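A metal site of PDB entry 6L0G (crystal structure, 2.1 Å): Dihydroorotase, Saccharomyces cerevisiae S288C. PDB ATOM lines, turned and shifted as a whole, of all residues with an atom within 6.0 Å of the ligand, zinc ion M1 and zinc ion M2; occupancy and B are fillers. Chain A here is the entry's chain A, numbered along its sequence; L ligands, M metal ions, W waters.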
ATOM      1  N   HIS A  14      -7.877   1.033 -16.118  1.00  0.00           N
ATOM      2  CA  HIS A  14      -8.547   0.011 -15.280  1.00  0.00           C
ATOM      3  C   HIS A  14      -7.626  -0.331 -14.107  1.00  0.00           C
ATOM      4  O   HIS A  14      -6.778  -1.219 -14.224  1.00  0.00           O
ATOM      5  CB  HIS A  14      -8.887  -1.216 -16.123  1.00  0.00           C
ATOM      6  CG  HIS A  14      -9.926  -2.121 -15.493  1.00  0.00           C
ATOM      7  ND1 HIS A  14     -10.996  -2.624 -16.197  1.00  0.00           N
ATOM      8  CD2 HIS A  14     -10.014  -2.644 -14.247  1.00  0.00           C
ATOM      9  CE1 HIS A  14     -11.716  -3.397 -15.398  1.00  0.00           C
ATOM     10  NE2 HIS A  14     -11.141  -3.435 -14.223  1.00  0.00           N
ATOM     11  N   HIS A  16      -7.102  -1.011  -9.787  1.00  0.00           N
ATOM     12  CA  HIS A  16      -7.554  -1.281  -8.417  1.00  0.00           C
ATOM     13  C   HIS A  16      -6.457  -0.922  -7.419  1.00  0.00           C
ATOM     14  O   HIS A  16      -5.340  -1.448  -7.513  1.00  0.00           O
ATOM     15  CB  HIS A  16      -7.943  -2.753  -8.249  1.00  0.00           C
ATOM     16  CG  HIS A  16      -9.102  -3.183  -9.116  1.00  0.00           C
ATOM     17  ND1 HIS A  16     -10.409  -3.111  -8.692  1.00  0.00           N
ATOM     18  CD2 HIS A  16      -9.133  -3.665 -10.374  1.00  0.00           C
ATOM     19  CE1 HIS A  16     -11.209  -3.538  -9.659  1.00  0.00           C
ATOM     20  NE2 HIS A  16     -10.456  -3.877 -10.693  1.00  0.00           N
ATOM     21  N   ARG A  18      -7.464  -0.549  -3.798  1.00  0.00           N
ATOM     22  CA  ARG A  18      -7.981  -1.017  -2.503  1.00  0.00           C
ATOM     23  C   ARG A  18      -8.062   0.150  -1.502  1.00  0.00           C
ATOM     24  O   ARG A  18      -8.375   1.288  -1.892  1.00  0.00           O
ATOM     25  CB  ARG A  18      -7.144  -2.193  -2.007  1.00  0.00           C
ATOM     26  CG  ARG A  18      -6.757  -3.243  -3.101  1.00  0.00           C
ATOM     27  CD  ARG A  18      -7.977  -3.910  -3.782  1.00  0.00           C
ATOM     28  NE  ARG A  18      -7.573  -5.107  -4.508  1.00  0.00           N
ATOM     29  CZ  ARG A  18      -8.286  -5.734  -5.438  1.00  0.00           C
ATOM     30  NH1 ARG A  18      -9.490  -5.280  -5.792  1.00  0.00           N
ATOM     31  NH2 ARG A  18      -7.784  -6.825  -6.030  1.00  0.00           N
ATOM     32  N   MET A  41     -11.145   1.938 -10.147  1.00  0.00           N
ATOM     33  CA  MET A  41     -12.373   1.155 -10.021  1.00  0.00           C
ATOM     34  C   MET A  41     -12.956   1.244  -8.607  1.00  0.00           C
ATOM     35  O   MET A  41     -12.239   1.541  -7.659  1.00  0.00           O
ATOM     36  CB  MET A  41     -12.080  -0.293 -10.402  1.00  0.00           C
ATOM     37  CG  MET A  41     -11.774  -0.445 -11.918  1.00  0.00           C
ATOM     38  SD  MET A  41     -13.197   0.111 -12.862  1.00  0.00           S
ATOM     39  CE  MET A  41     -12.707  -0.008 -14.567  1.00  0.00           C
ATOM     40  N   ASN A  43     -14.863  -1.109  -6.608  1.00  0.00           N
ATOM     41  CA  ASN A  43     -15.361  -2.309  -5.927  1.00  0.00           C
ATOM     42  C   ASN A  43     -14.664  -2.482  -4.560  1.00  0.00           C
ATOM     43  O   ASN A  43     -14.018  -3.484  -4.270  1.00  0.00           O
ATOM     44  CB  ASN A  43     -15.198  -3.541  -6.814  1.00  0.00           C
ATOM     45  CG  ASN A  43     -13.743  -3.862  -7.135  1.00  0.00           C
ATOM     46  OD1 ASN A  43     -12.891  -2.981  -7.123  1.00  0.00           O
ATOM     47  ND2 ASN A  43     -13.454  -5.135  -7.406  1.00  0.00           N
ATOM     48  N   KCX A  98     -19.053   1.806 -13.153  1.00  0.00           N
ATOM     49  CA  KCX A  98     -18.567   0.466 -13.458  1.00  0.00           C
ATOM     50  CB  KCX A  98     -17.261   0.160 -12.715  1.00  0.00           C
ATOM     51  CG  KCX A  98     -16.837  -1.305 -12.807  1.00  0.00           C
ATOM     52  CD  KCX A  98     -16.424  -1.649 -14.239  1.00  0.00           C
ATOM     53  CE  KCX A  98     -15.765  -3.020 -14.324  1.00  0.00           C
ATOM     54  NZ  KCX A  98     -14.704  -3.058 -13.298  1.00  0.00           N
ATOM     55  C   KCX A  98     -19.593  -0.586 -13.092  1.00  0.00           C
ATOM     56  O   KCX A  98     -20.068  -0.623 -11.958  1.00  0.00           O
ATOM     57  CX  KCX A  98     -13.921  -4.122 -13.161  1.00  0.00           C
ATOM     58  OQ1 KCX A  98     -13.061  -4.123 -12.271  1.00  0.00           O
ATOM     59  OQ2 KCX A  98     -14.073  -5.123 -13.879  1.00  0.00           O
ATOM     60  N   TYR A 100     -20.453  -4.448 -12.336  1.00  0.00           N
ATOM     61  CA  TYR A 100     -20.063  -5.804 -11.985  1.00  0.00           C
ATOM     62  C   TYR A 100     -21.295  -6.703 -11.993  1.00  0.00           C
ATOM     63  O   TYR A 100     -22.241  -6.418 -11.261  1.00  0.00           O
ATOM     64  CB  TYR A 100     -19.398  -5.859 -10.585  1.00  0.00           C
ATOM     65  CG  TYR A 100     -18.085  -5.100 -10.486  1.00  0.00           C
ATOM     66  CD1 TYR A 100     -16.910  -5.680 -10.894  1.00  0.00           C
ATOM     67  CD2 TYR A 100     -18.059  -3.790  -9.995  1.00  0.00           C
ATOM     68  CE1 TYR A 100     -15.717  -4.979 -10.800  1.00  0.00           C
ATOM     69  CE2 TYR A 100     -16.878  -3.095  -9.905  1.00  0.00           C
ATOM     70  CZ  TYR A 100     -15.701  -3.686 -10.305  1.00  0.00           C
ATOM     71  OH  TYR A 100     -14.523  -2.979 -10.224  1.00  0.00           O
ATOM     72  N   VAL A 104     -19.471 -12.589 -10.071  1.00  0.00           N
ATOM     73  CA  VAL A 104     -18.495 -13.077 -11.051  1.00  0.00           C
ATOM     74  C   VAL A 104     -17.053 -12.738 -10.674  1.00  0.00           C
ATOM     75  O   VAL A 104     -16.134 -13.366 -11.231  1.00  0.00           O
ATOM     76  CB  VAL A 104     -18.776 -12.575 -12.481  1.00  0.00           C
ATOM     77  CG1 VAL A 104     -20.168 -13.019 -12.951  1.00  0.00           C
ATOM     78  CG2 VAL A 104     -18.636 -11.059 -12.583  1.00  0.00           C
ATOM     79  N   THR A 105     -16.820 -11.819  -9.740  1.00  0.00           N
ATOM     80  CA  THR A 105     -15.437 -11.456  -9.428  1.00  0.00           C
ATOM     81  C   THR A 105     -15.352 -10.786  -8.057  1.00  0.00           C
ATOM     82  O   THR A 105     -16.306 -10.805  -7.265  1.00  0.00           O
ATOM     83  CB  THR A 105     -14.868 -10.562 -10.535  1.00  0.00           C
ATOM     84  OG1 THR A 105     -13.460 -10.453 -10.379  1.00  0.00           O
ATOM     85  CG2 THR A 105     -15.497  -9.185 -10.512  1.00  0.00           C
ATOM     86  N   THR A 106     -14.170 -10.232  -7.756  1.00  0.00           N
ATOM     87  CA  THR A 106     -13.878  -9.662  -6.445  1.00  0.00           C
ATOM     88  C   THR A 106     -14.865  -8.543  -6.088  1.00  0.00           C
ATOM     89  O   THR A 106     -15.040  -7.588  -6.851  1.00  0.00           O
ATOM     90  CB  THR A 106     -12.455  -9.089  -6.421  1.00  0.00           C
ATOM     91  OG1 THR A 106     -11.496 -10.125  -6.738  1.00  0.00           O
ATOM     92  CG2 THR A 106     -12.132  -8.518  -5.066  1.00  0.00           C
ATOM     93  N   ASN A 107     -15.479  -8.664  -4.904  1.00  0.00           N
ATOM     94  CA  ASN A 107     -16.394  -7.651  -4.362  1.00  0.00           C
ATOM     95  C   ASN A 107     -17.512  -7.310  -5.345  1.00  0.00           C
ATOM     96  O   ASN A 107     -17.868  -6.139  -5.558  1.00  0.00           O
ATOM     97  CB  ASN A 107     -15.626  -6.401  -3.941  1.00  0.00           C
ATOM     98  CG  ASN A 107     -14.764  -6.648  -2.702  1.00  0.00           C
ATOM     99  OD1 ASN A 107     -15.003  -7.593  -1.960  1.00  0.00           O
ATOM    100  ND2 ASN A 107     -13.748  -5.797  -2.491  1.00  0.00           N
ATOM    101  N   HIS A 137     -17.844  -5.032 -16.769  1.00  0.00           N
ATOM    102  CA  HIS A 137     -17.189  -6.327 -16.637  1.00  0.00           C
ATOM    103  C   HIS A 137     -18.121  -7.292 -17.349  1.00  0.00           C
ATOM    104  O   HIS A 137     -19.110  -7.768 -16.796  1.00  0.00           O
ATOM    105  CB  HIS A 137     -16.963  -6.707 -15.179  1.00  0.00           C
ATOM    106  CG  HIS A 137     -16.288  -8.043 -15.012  1.00  0.00           C
ATOM    107  ND1 HIS A 137     -15.144  -8.212 -14.240  1.00  0.00           N
ATOM    108  CD2 HIS A 137     -16.585  -9.262 -15.517  1.00  0.00           C
ATOM    109  CE1 HIS A 137     -14.786  -9.485 -14.271  1.00  0.00           C
ATOM    110  NE2 HIS A 137     -15.650 -10.145 -15.030  1.00  0.00           N
ATOM    111  N   GLU A 179     -14.599  -3.906 -20.638  1.00  0.00           N
ATOM    112  CA  GLU A 179     -13.327  -3.964 -19.938  1.00  0.00           C
ATOM    113  C   GLU A 179     -12.658  -5.325 -20.141  1.00  0.00           C
ATOM    114  O   GLU A 179     -13.318  -6.339 -20.389  1.00  0.00           O
ATOM    115  CB  GLU A 179     -13.516  -3.731 -18.432  1.00  0.00           C
ATOM    116  CG  GLU A 179     -14.042  -2.344 -18.061  1.00  0.00           C
ATOM    117  CD  GLU A 179     -13.065  -1.231 -18.387  1.00  0.00           C
ATOM    118  OE1 GLU A 179     -11.842  -1.505 -18.424  1.00  0.00           O
ATOM    119  OE2 GLU A 179     -13.526  -0.080 -18.604  1.00  0.00           O
ATOM    120  N   HIS A 180     -11.322  -5.323 -20.037  1.00  0.00           N
ATOM    121  CA  HIS A 180     -10.464  -6.501 -20.090  1.00  0.00           C
ATOM    122  C   HIS A 180     -11.021  -7.614 -20.965  1.00  0.00           C
ATOM    123  O   HIS A 180     -11.463  -8.653 -20.456  1.00  0.00           O
ATOM    124  CB  HIS A 180     -10.137  -7.020 -18.673  1.00  0.00           C
ATOM    125  CG  HIS A 180     -11.298  -7.039 -17.712  1.00  0.00           C
ATOM    126  ND1 HIS A 180     -12.556  -7.475 -18.075  1.00  0.00           N
ATOM    127  CD2 HIS A 180     -11.376  -6.753 -16.401  1.00  0.00           C
ATOM    128  CE1 HIS A 180     -13.361  -7.421 -17.032  1.00  0.00           C
ATOM    129  NE2 HIS A 180     -12.675  -6.974 -16.005  1.00  0.00           N
ATOM    130  N   CYS A 229      -7.436 -14.907 -12.753  1.00  0.00           N
ATOM    131  CA  CYS A 229      -8.126 -13.632 -12.712  1.00  0.00           C
ATOM    132  C   CYS A 229      -9.461 -13.809 -13.413  1.00  0.00           C
ATOM    133  O   CYS A 229      -9.695 -14.832 -14.066  1.00  0.00           O
ATOM    134  CB  CYS A 229      -7.268 -12.529 -13.371  1.00  0.00           C
ATOM    135  SG  CYS A 229      -7.078 -12.764 -15.164  1.00  0.00           S
ATOM    136  N   LYS A 230     -10.332 -12.780 -13.311  1.00  0.00           N
ATOM    137  CA  LYS A 230     -11.539 -12.734 -14.120  1.00  0.00           C
ATOM    138  C   LYS A 230     -11.481 -11.555 -15.096  1.00  0.00           C
ATOM    139  O   LYS A 230     -10.992 -10.487 -14.724  1.00  0.00           O
ATOM    140  CB  LYS A 230     -12.779 -12.611 -13.236  1.00  0.00           C
ATOM    141  CG  LYS A 230     -13.038 -13.807 -12.314  1.00  0.00           C
ATOM    142  CD  LYS A 230     -13.097 -15.102 -13.109  1.00  0.00           C
ATOM    143  CE  LYS A 230     -14.463 -15.247 -13.743  1.00  0.00           C
ATOM    144  NZ  LYS A 230     -15.495 -15.650 -12.708  1.00  0.00           N
ATOM    145  N   PRO A 231     -11.947 -11.715 -16.353  1.00  0.00           N
ATOM    146  CA  PRO A 231     -12.266 -13.014 -16.985  1.00  0.00           C
ATOM    147  C   PRO A 231     -11.012 -13.878 -17.118  1.00  0.00           C
ATOM    148  O   PRO A 231      -9.900 -13.326 -17.214  1.00  0.00           O
ATOM    149  CB  PRO A 231     -12.832 -12.615 -18.369  1.00  0.00           C
ATOM    150  CG  PRO A 231     -12.981 -11.077 -18.327  1.00  0.00           C
ATOM    151  CD  PRO A 231     -11.923 -10.639 -17.358  1.00  0.00           C
ATOM    152  N   ASP A 258      -6.227  -3.693 -15.335  1.00  0.00           N
ATOM    153  CA  ASP A 258      -6.928  -4.438 -14.305  1.00  0.00           C
ATOM    154  C   ASP A 258      -5.953  -4.990 -13.269  1.00  0.00           C
ATOM    155  O   ASP A 258      -6.083  -6.116 -12.788  1.00  0.00           O
ATOM    156  CB  ASP A 258      -7.773  -5.578 -14.902  1.00  0.00           C
ATOM    157  CG  ASP A 258      -8.733  -6.213 -13.875  1.00  0.00           C
ATOM    158  OD1 ASP A 258      -9.039  -5.569 -12.856  1.00  0.00           O
ATOM    159  OD2 ASP A 258      -9.158  -7.377 -14.099  1.00  0.00           O
ATOM    160  N   SER A 259      -4.943  -4.184 -12.931  1.00  0.00           N
ATOM    161  CA  SER A 259      -4.061  -4.575 -11.835  1.00  0.00           C
ATOM    162  C   SER A 259      -4.889  -4.668 -10.554  1.00  0.00           C
ATOM    163  O   SER A 259      -5.578  -3.716 -10.188  1.00  0.00           O
ATOM    164  CB  SER A 259      -2.922  -3.582 -11.675  1.00  0.00           C
ATOM    165  OG  SER A 259      -2.143  -3.891 -10.533  1.00  0.00           O
ATOM    166  N   ALA A 260      -4.858  -5.843  -9.930  1.00  0.00           N
ATOM    167  CA  ALA A 260      -5.771  -6.199  -8.832  1.00  0.00           C
ATOM    168  C   ALA A 260      -4.978  -6.785  -7.671  1.00  0.00           C
ATOM    169  O   ALA A 260      -4.771  -8.009  -7.602  1.00  0.00           O
ATOM    170  CB  ALA A 260      -6.829  -7.179  -9.314  1.00  0.00           C
ATOM    171  N   PRO A 261      -4.522  -5.953  -6.730  1.00  0.00           N
ATOM    172  CA  PRO A 261      -3.655  -6.458  -5.658  1.00  0.00           C
ATOM    173  C   PRO A 261      -4.413  -7.315  -4.654  1.00  0.00           C
ATOM    174  O   PRO A 261      -5.503  -6.968  -4.206  1.00  0.00           O
ATOM    175  CB  PRO A 261      -3.112  -5.195  -4.995  1.00  0.00           C
ATOM    176  CG  PRO A 261      -3.995  -4.095  -5.413  1.00  0.00           C
ATOM    177  CD  PRO A 261      -4.767  -4.499  -6.623  1.00  0.00           C
ATOM    178  N   HIS A 262      -3.799  -8.449  -4.284  1.00  0.00           N
ATOM    179  CA  HIS A 262      -4.257  -9.321  -3.210  1.00  0.00           C
ATOM    180  C   HIS A 262      -3.068  -9.727  -2.356  1.00  0.00           C
ATOM    181  O   HIS A 262      -1.990 -10.036  -2.898  1.00  0.00           O
ATOM    182  CB  HIS A 262      -4.936 -10.578  -3.767  1.00  0.00           C
ATOM    183  CG  HIS A 262      -6.223 -10.301  -4.482  1.00  0.00           C
ATOM    184  ND1 HIS A 262      -7.379  -9.980  -3.798  1.00  0.00           N
ATOM    185  CD2 HIS A 262      -6.537 -10.290  -5.790  1.00  0.00           C
ATOM    186  CE1 HIS A 262      -8.360  -9.774  -4.671  1.00  0.00           C
ATOM    187  NE2 HIS A 262      -7.873  -9.959  -5.883  1.00  0.00           N
ATOM    188  N   ALA A 275      -9.515 -13.723  -7.293  1.00  0.00           N
ATOM    189  CA  ALA A 275      -9.219 -13.469  -8.688  1.00  0.00           C
ATOM    190  C   ALA A 275      -8.478 -12.147  -8.836  1.00  0.00           C
ATOM    191  O   ALA A 275      -8.884 -11.129  -8.261  1.00  0.00           O
ATOM    192  CB  ALA A 275     -10.509 -13.433  -9.506  1.00  0.00           C
ATOM    193  N   GLY A 276      -7.430 -12.151  -9.634  1.00  0.00           N
ATOM    194  CA  GLY A 276      -6.730 -10.911  -9.919  1.00  0.00           C
ATOM    195  C   GLY A 276      -5.236 -11.038 -10.075  1.00  0.00           C
ATOM    196  O   GLY A 276      -4.574 -11.797  -9.346  1.00  0.00           O
ATOM    197  N   VAL A 277      -4.693 -10.292 -11.037  1.00  0.00           N
ATOM    198  CA  VAL A 277      -3.265 -10.273 -11.330  1.00  0.00           C
ATOM    199  C   VAL A 277      -2.761  -8.879 -11.000  1.00  0.00           C
ATOM    200  O   VAL A 277      -3.386  -7.887 -11.415  1.00  0.00           O
ATOM    201  CB  VAL A 277      -3.000 -10.630 -12.809  1.00  0.00           C
ATOM    202  CG1 VAL A 277      -1.518 -10.475 -13.157  1.00  0.00           C
ATOM    203  CG2 VAL A 277      -3.469 -12.053 -13.114  1.00  0.00           C
HETATM  204  C1  LIG L   1     -11.870  -7.978 -11.547  1.00  0.00           C
HETATM  205  O1  LIG L   1     -11.572  -6.983 -12.266  1.00  0.00           O
HETATM  206  O2  LIG L   1     -12.606  -8.838 -12.060  1.00  0.00           O
HETATM  207  C2  LIG L   1     -11.359  -8.155 -10.099  1.00  0.00           C
HETATM  208  O3  LIG L   1     -10.458  -9.218  -9.888  1.00  0.00           O
HETATM  209  C3  LIG L   1     -10.538  -6.964  -9.768  1.00  0.00           C
HETATM  210  C4  LIG L   1     -10.397  -7.086  -8.273  1.00  0.00           C
HETATM  211  O4  LIG L   1      -9.843  -8.094  -7.724  1.00  0.00           O
HETATM  212  O5  LIG L   1     -10.851  -6.100  -7.645  1.00  0.00           O
HETATM  213 ZN    ZN M   1     -13.418  -6.936 -14.009  1.00  0.00          ZN
HETATM  214 ZN    ZN M   2     -10.994  -4.759 -12.550  1.00  0.00          ZN
HETATM  215  O   HOH W   1      -9.327 -10.016 -12.325  1.00  0.00           O
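Water W1 lies within hydrogen-bond range of an oxygen (O3) of the ligand (2.8 Å), the backbone carbonyl oxygen of Lys 230 (3.0 Å) and the side-chain carboxylate of Asp 258 (3.2 Å).
Zinc ion M2 is bound by a ring nitrogen (NE2) of His 16 (2.1 Å), a ring nitrogen (NE2) of His 14 (2.1 Å), the side-chain carboxylate of Asp 258 (2.1 Å), OQ1 of KCX 98 (2.2 Å) and an oxygen (O1) of the ligand (2.3 Å).
An oxygen (O2) of the ligand lies within hydrogen-bond range of the side-chain hydroxyl of Thr 105 (2.5 Å).
The side-chain hydroxyl (OG1) of Thr 106 sits at hydrogen-bond distance from an oxygen (O4) of the ligand, 2.8 Å away.
O5 of the ligand is in salt-bridge range of NH1 of Arg 18 (2.4 Å).
The side-chain amide nitrogen of Asn 43 lies within hydrogen-bond range of an oxygen (O5) of the ligand, 2.8 Å away.
NE2 of His 262 lies within hydrogen-bond range of O4 of the ligand (3.3 Å).
An oxygen (O3) of the ligand sits at hydrogen-bond distance from the backbone carbonyl oxygen of Ala 275 (3.0 Å).
Lys 230 touches the ligand.
Ala 260 touches the ligand.
Hydrophobic or aromatic side chains that line the ligand: His 16, His 137, Ala 260 and His 262.
Of the 25 residues printed, 13 come within 4 Å of the ligand.
The nearest printed residue that does not touch the ligand is His 14 (4.1 Å).
Zinc ion M1 is bound by OQ2 of KCX 98, a ring nitrogen (NE2) of His 180, a ring nitrogen (ND1) of His 137 and an oxygen (O1) of the ligand.
Zinc ion M1 has four donor atoms within binding distance.
Slightly farther from zinc ion M1 lies an oxygen (O2) of the ligand (2.8 Å).
The backbone NH (N) of Ala 260 lies within hydrogen-bond range of the backbone carbonyl oxygen (O) of Val 277, 2.9 Å away.
The guanidinium group of Arg 18 is in hydrogen-bond range of a ring nitrogen (NE2) of His 262, 3.1 Å away.
O of Ala 275 is in hydrogen-bond range of NE2 of His 262, at 2.8 Å.
ND1 of His 16 sits at hydrogen-bond distance from OD1 of Asn 43 (2.9 Å).
The backbone carbonyl oxygen (O) of Ser 259 lies within hydrogen-bond range of the backbone NH (N) of His 16, 3.1 Å away.
ND2 of Asn 43 lies within hydrogen-bond range of O of Thr 106 (3.0 Å).
NZ of KCX 98 lies within hydrogen-bond range of the side-chain hydroxyl (OH) of Tyr 100, at 3.1 Å.
NE of Arg 18 sits at hydrogen-bond distance from O of Pro 261 (2.8 Å).
Of the 25 residues printed, 4 come within 4 Å of zinc ion M2.
Along chain A the residues within 4 Å of zinc ion M2 span positions 14 to 258.
The nearest printed residue that does not touch zinc ion M2 is His 180 (4.4 Å).
Three residues have an atom within 4 Å of zinc ion M1: KCX 98, His 137 and His 180.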
